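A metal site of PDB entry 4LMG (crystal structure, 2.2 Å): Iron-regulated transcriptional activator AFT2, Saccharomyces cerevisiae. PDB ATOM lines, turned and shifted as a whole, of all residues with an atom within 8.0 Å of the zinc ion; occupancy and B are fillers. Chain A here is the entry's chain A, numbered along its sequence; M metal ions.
Merely in contact with the zinc ion: Phe 75 (3.9 Å).
Within 4 Å of the zinc ion: Cys 50, Cys 73, Phe 75, His 97 and His 99.
The nearest printed residue that does not touch the zinc ion is Ser 98 (4.8 Å).
The zinc ion is bound by NE2 of His 99 (2.0 Å), ND1 of His 97 (2.1 Å), SG of Cys 73 (2.3 Å) and SG of Cys 50 (2.3 Å).
The backbone NH (N) of Cys 73 lies close to the side-chain hydroxyl (OG) of Ser 98, 3.5 Å away.
The backbone NH of Phe 75 lies close to the side-chain sulfur of Cys 73, 3.6 Å away.
The guanidinium group of Arg 76 is in hydrogen-bond range of the backbone carbonyl oxygen of Cys 73, at 2.8 Å.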
ATOM      1  N   GLY A  33     -21.916 -24.826 -21.874  1.00  0.00           N
ATOM      2  CA  GLY A  33     -21.122 -23.638 -22.122  1.00  0.00           C
ATOM      3  C   GLY A  33     -20.040 -23.455 -21.085  1.00  0.00           C
ATOM      4  O   GLY A  33     -19.586 -22.342 -20.808  1.00  0.00           O
ATOM      5  N   ILE A  34     -19.614 -24.572 -20.486  1.00  0.00           N
ATOM      6  CA  ILE A  34     -18.591 -24.539 -19.457  1.00  0.00           C
ATOM      7  C   ILE A  34     -17.346 -25.262 -19.926  1.00  0.00           C
ATOM      8  O   ILE A  34     -17.392 -26.439 -20.280  1.00  0.00           O
ATOM      9  CB  ILE A  34     -19.096 -25.175 -18.142  1.00  0.00           C
ATOM     10  CG1 ILE A  34     -20.269 -24.376 -17.601  1.00  0.00           C
ATOM     11  CG2 ILE A  34     -17.968 -25.241 -17.114  1.00  0.00           C
ATOM     12  CD1 ILE A  34     -20.934 -24.994 -16.381  1.00  0.00           C
ATOM     13  N   ASP A  35     -16.222 -24.535 -19.936  1.00  0.00           N
ATOM     14  CA  ASP A  35     -14.955 -25.044 -20.450  1.00  0.00           C
ATOM     15  C   ASP A  35     -14.026 -25.353 -19.272  1.00  0.00           C
ATOM     16  O   ASP A  35     -13.400 -24.455 -18.720  1.00  0.00           O
ATOM     17  CB  ASP A  35     -14.320 -23.991 -21.363  1.00  0.00           C
ATOM     18  CG  ASP A  35     -13.092 -24.512 -22.097  1.00  0.00           C
ATOM     19  OD1 ASP A  35     -12.608 -25.613 -21.771  1.00  0.00           O
ATOM     20  OD2 ASP A  35     -12.619 -23.821 -23.020  1.00  0.00           O
ATOM     21  N   LYS A  49     -11.526 -26.118 -12.932  1.00  0.00           N
ATOM     22  CA  LYS A  49     -12.167 -24.804 -12.943  1.00  0.00           C
ATOM     23  C   LYS A  49     -12.409 -24.347 -14.372  1.00  0.00           C
ATOM     24  O   LYS A  49     -12.022 -25.035 -15.325  1.00  0.00           O
ATOM     25  CB  LYS A  49     -11.320 -23.777 -12.188  1.00  0.00           C
ATOM     26  CG  LYS A  49      -9.944 -23.540 -12.804  1.00  0.00           C
ATOM     27  CD  LYS A  49      -9.160 -22.533 -11.980  1.00  0.00           C
ATOM     28  CE  LYS A  49      -7.761 -22.334 -12.528  1.00  0.00           C
ATOM     29  NZ  LYS A  49      -6.944 -21.510 -11.597  1.00  0.00           N
ATOM     30  N   CYS A  50     -13.047 -23.192 -14.529  1.00  0.00           N
ATOM     31  CA  CYS A  50     -13.287 -22.652 -15.862  1.00  0.00           C
ATOM     32  C   CYS A  50     -11.988 -22.135 -16.468  1.00  0.00           C
ATOM     33  O   CYS A  50     -11.210 -21.467 -15.794  1.00  0.00           O
ATOM     34  CB  CYS A  50     -14.318 -21.510 -15.816  1.00  0.00           C
ATOM     35  SG  CYS A  50     -16.026 -22.052 -15.557  1.00  0.00           S
ATOM     36  N   ARG A  51     -11.763 -22.450 -17.734  1.00  0.00           N
ATOM     37  CA  ARG A  51     -10.623 -21.887 -18.442  1.00  0.00           C
ATOM     38  C   ARG A  51     -10.627 -20.378 -18.247  1.00  0.00           C
ATOM     39  O   ARG A  51     -11.682 -19.741 -18.283  1.00  0.00           O
ATOM     40  CB  ARG A  51     -10.677 -22.223 -19.928  1.00  0.00           C
ATOM     41  CG  ARG A  51      -9.468 -21.696 -20.691  1.00  0.00           C
ATOM     42  CD  ARG A  51      -9.596 -21.977 -22.173  1.00  0.00           C
ATOM     43  NE  ARG A  51      -9.954 -23.369 -22.416  1.00  0.00           N
ATOM     44  CZ  ARG A  51      -9.100 -24.382 -22.360  1.00  0.00           C
ATOM     45  NH1 ARG A  51      -7.822 -24.166 -22.068  1.00  0.00           N
ATOM     46  NH2 ARG A  51      -9.523 -25.610 -22.596  1.00  0.00           N
ATOM     47  N   ALA A  72     -12.099 -13.278 -12.209  1.00  0.00           N
ATOM     48  CA  ALA A  72     -11.846 -14.674 -11.866  1.00  0.00           C
ATOM     49  C   ALA A  72     -13.134 -15.391 -11.470  1.00  0.00           C
ATOM     50  O   ALA A  72     -13.915 -14.878 -10.664  1.00  0.00           O
ATOM     51  CB  ALA A  72     -10.812 -14.780 -10.767  1.00  0.00           C
ATOM     52  N   CYS A  73     -13.347 -16.572 -12.038  1.00  0.00           N
ATOM     53  CA  CYS A  73     -14.559 -17.344 -11.758  1.00  0.00           C
ATOM     54  C   CYS A  73     -14.345 -18.322 -10.612  1.00  0.00           C
ATOM     55  O   CYS A  73     -13.375 -19.068 -10.601  1.00  0.00           O
ATOM     56  CB  CYS A  73     -15.002 -18.097 -13.008  1.00  0.00           C
ATOM     57  SG  CYS A  73     -16.527 -19.018 -12.797  1.00  0.00           S
ATOM     58  N   PRO A  74     -15.283 -18.326  -9.647  1.00  0.00           N
ATOM     59  CA  PRO A  74     -15.197 -19.125  -8.425  1.00  0.00           C
ATOM     60  C   PRO A  74     -15.597 -20.586  -8.629  1.00  0.00           C
ATOM     61  O   PRO A  74     -15.267 -21.426  -7.778  1.00  0.00           O
ATOM     62  CB  PRO A  74     -16.210 -18.441  -7.504  1.00  0.00           C
ATOM     63  CG  PRO A  74     -17.243 -17.913  -8.436  1.00  0.00           C
ATOM     64  CD  PRO A  74     -16.499 -17.484  -9.675  1.00  0.00           C
ATOM     65  N   PHE A  75     -16.289 -20.878  -9.717  1.00  0.00           N
ATOM     66  CA  PHE A  75     -16.721 -22.243 -10.025  1.00  0.00           C
ATOM     67  C   PHE A  75     -15.590 -23.245  -9.845  1.00  0.00           C
ATOM     68  O   PHE A  75     -14.473 -23.026 -10.323  1.00  0.00           O
ATOM     69  CB  PHE A  75     -17.262 -22.312 -11.454  1.00  0.00           C
ATOM     70  CG  PHE A  75     -17.762 -23.677 -11.857  1.00  0.00           C
ATOM     71  CD1 PHE A  75     -16.951 -24.537 -12.582  1.00  0.00           C
ATOM     72  CD2 PHE A  75     -19.042 -24.098 -11.528  1.00  0.00           C
ATOM     73  CE1 PHE A  75     -17.404 -25.785 -12.966  1.00  0.00           C
ATOM     74  CE2 PHE A  75     -19.497 -25.338 -11.906  1.00  0.00           C
ATOM     75  CZ  PHE A  75     -18.688 -26.189 -12.626  1.00  0.00           C
ATOM     76  N   ARG A  76     -15.879 -24.344  -9.152  1.00  0.00           N
ATOM     77  CA  ARG A  76     -14.872 -25.378  -8.905  1.00  0.00           C
ATOM     78  C   ARG A  76     -15.472 -26.779  -8.924  1.00  0.00           C
ATOM     79  O   ARG A  76     -16.551 -27.020  -8.400  1.00  0.00           O
ATOM     80  CB  ARG A  76     -14.172 -25.152  -7.559  1.00  0.00           C
ATOM     81  CG  ARG A  76     -13.207 -23.985  -7.535  1.00  0.00           C
ATOM     82  CD  ARG A  76     -12.118 -24.136  -8.590  1.00  0.00           C
ATOM     83  NE  ARG A  76     -11.090 -23.109  -8.458  1.00  0.00           N
ATOM     84  CZ  ARG A  76     -11.230 -21.846  -8.860  1.00  0.00           C
ATOM     85  NH1 ARG A  76     -12.374 -21.448  -9.413  1.00  0.00           N
ATOM     86  NH2 ARG A  76     -10.240 -20.985  -8.704  1.00  0.00           N
ATOM     87  N   ASN A  94     -19.252 -23.747  -5.531  1.00  0.00           N
ATOM     88  CA  ASN A  94     -19.522 -22.415  -6.061  1.00  0.00           C
ATOM     89  C   ASN A  94     -20.111 -22.471  -7.469  1.00  0.00           C
ATOM     90  O   ASN A  94     -19.469 -22.070  -8.431  1.00  0.00           O
ATOM     91  CB  ASN A  94     -18.258 -21.562  -6.056  1.00  0.00           C
ATOM     92  CG  ASN A  94     -17.845 -21.147  -4.661  1.00  0.00           C
ATOM     93  OD1 ASN A  94     -16.764 -21.511  -4.179  1.00  0.00           O
ATOM     94  ND2 ASN A  94     -18.692 -20.382  -3.987  1.00  0.00           N
ATOM     95  N   ASN A  95     -21.342 -22.961  -7.562  1.00  0.00           N
ATOM     96  CA  ASN A  95     -21.982 -23.144  -8.861  1.00  0.00           C
ATOM     97  C   ASN A  95     -22.230 -21.835  -9.612  1.00  0.00           C
ATOM     98  O   ASN A  95     -22.812 -21.827 -10.687  1.00  0.00           O
ATOM     99  CB  ASN A  95     -23.297 -23.912  -8.695  1.00  0.00           C
ATOM    100  CG  ASN A  95     -23.859 -24.383 -10.009  1.00  0.00           C
ATOM    101  OD1 ASN A  95     -24.924 -23.944 -10.436  1.00  0.00           O
ATOM    102  ND2 ASN A  95     -23.137 -25.271 -10.680  1.00  0.00           N
ATOM    103  N   ILE A  96     -21.763 -20.728  -9.023  1.00  0.00           N
ATOM    104  CA  ILE A  96     -21.943 -19.412  -9.613  1.00  0.00           C
ATOM    105  C   ILE A  96     -20.757 -19.047 -10.506  1.00  0.00           C
ATOM    106  O   ILE A  96     -19.607 -19.311 -10.159  1.00  0.00           O
ATOM    107  CB  ILE A  96     -22.085 -18.332  -8.542  1.00  0.00           C
ATOM    108  CG1 ILE A  96     -23.152 -18.736  -7.516  1.00  0.00           C
ATOM    109  CG2 ILE A  96     -22.411 -16.987  -9.166  1.00  0.00           C
ATOM    110  CD1 ILE A  96     -23.278 -17.769  -6.356  1.00  0.00           C
ATOM    111  N   HIS A  97     -21.041 -18.454 -11.653  1.00  0.00           N
ATOM    112  CA  HIS A  97     -19.995 -18.014 -12.572  1.00  0.00           C
ATOM    113  C   HIS A  97     -19.919 -16.497 -12.649  1.00  0.00           C
ATOM    114  O   HIS A  97     -20.912 -15.800 -12.439  1.00  0.00           O
ATOM    115  CB  HIS A  97     -20.220 -18.598 -13.967  1.00  0.00           C
ATOM    116  CG  HIS A  97     -20.088 -20.095 -14.029  1.00  0.00           C
ATOM    117  ND1 HIS A  97     -18.898 -20.721 -14.347  1.00  0.00           N
ATOM    118  CD2 HIS A  97     -20.987 -21.076 -13.818  1.00  0.00           C
ATOM    119  CE1 HIS A  97     -19.082 -22.028 -14.331  1.00  0.00           C
ATOM    120  NE2 HIS A  97     -20.340 -22.271 -14.010  1.00  0.00           N
ATOM    121  N   SER A  98     -18.735 -15.991 -12.971  1.00  0.00           N
ATOM    122  CA  SER A  98     -18.513 -14.553 -13.085  1.00  0.00           C
ATOM    123  C   SER A  98     -18.493 -14.154 -14.553  1.00  0.00           C
ATOM    124  O   SER A  98     -17.979 -13.081 -14.912  1.00  0.00           O
ATOM    125  CB  SER A  98     -17.193 -14.170 -12.440  1.00  0.00           C
ATOM    126  OG  SER A  98     -16.096 -14.731 -13.152  1.00  0.00           O
ATOM    127  N   HIS A  99     -19.062 -15.005 -15.406  1.00  0.00           N
ATOM    128  CA  HIS A  99     -18.977 -14.804 -16.844  1.00  0.00           C
ATOM    129  C   HIS A  99     -20.111 -15.533 -17.550  1.00  0.00           C
ATOM    130  O   HIS A  99     -20.750 -16.415 -16.982  1.00  0.00           O
ATOM    131  CB  HIS A  99     -17.637 -15.338 -17.354  1.00  0.00           C
ATOM    132  CG  HIS A  99     -17.414 -16.784 -17.055  1.00  0.00           C
ATOM    133  ND1 HIS A  99     -17.731 -17.792 -17.944  1.00  0.00           N
ATOM    134  CD2 HIS A  99     -16.910 -17.395 -15.946  1.00  0.00           C
ATOM    135  CE1 HIS A  99     -17.424 -18.957 -17.401  1.00  0.00           C
ATOM    136  NE2 HIS A  99     -16.935 -18.746 -16.190  1.00  0.00           N
ATOM    137  N   GLU A 100     -20.351 -15.151 -18.804  1.00  0.00           N
ATOM    138  CA  GLU A 100     -21.398 -15.786 -19.595  1.00  0.00           C
ATOM    139  C   GLU A 100     -20.944 -17.151 -20.086  1.00  0.00           C
ATOM    140  O   GLU A 100     -19.756 -17.367 -20.332  1.00  0.00           O
ATOM    141  CB  GLU A 100     -21.777 -14.886 -20.780  1.00  0.00           C
ATOM    142  CG  GLU A 100     -22.258 -13.507 -20.375  1.00  0.00           C
ATOM    143  CD  GLU A 100     -22.603 -12.631 -21.568  1.00  0.00           C
ATOM    144  OE1 GLU A 100     -22.632 -13.161 -22.706  1.00  0.00           O
ATOM    145  OE2 GLU A 100     -22.825 -11.420 -21.367  1.00  0.00           O
ATOM    146  N   LEU A 101     -21.893 -18.064 -20.204  1.00  0.00           N
ATOM    147  CA  LEU A 101     -21.593 -19.416 -20.668  1.00  0.00           C
ATOM    148  C   LEU A 101     -21.999 -19.557 -22.133  1.00  0.00           C
ATOM    149  O   LEU A 101     -23.186 -19.667 -22.451  1.00  0.00           O
ATOM    150  CB  LEU A 101     -22.324 -20.448 -19.818  1.00  0.00           C
ATOM    151  CG  LEU A 101     -22.142 -20.322 -18.303  1.00  0.00           C
ATOM    152  CD1 LEU A 101     -22.793 -21.484 -17.583  1.00  0.00           C
ATOM    153  CD2 LEU A 101     -20.665 -20.233 -17.942  1.00  0.00           C
HETATM  154 ZN    ZN M   1     -16.950 -20.147 -14.715  1.00  0.00          ZN
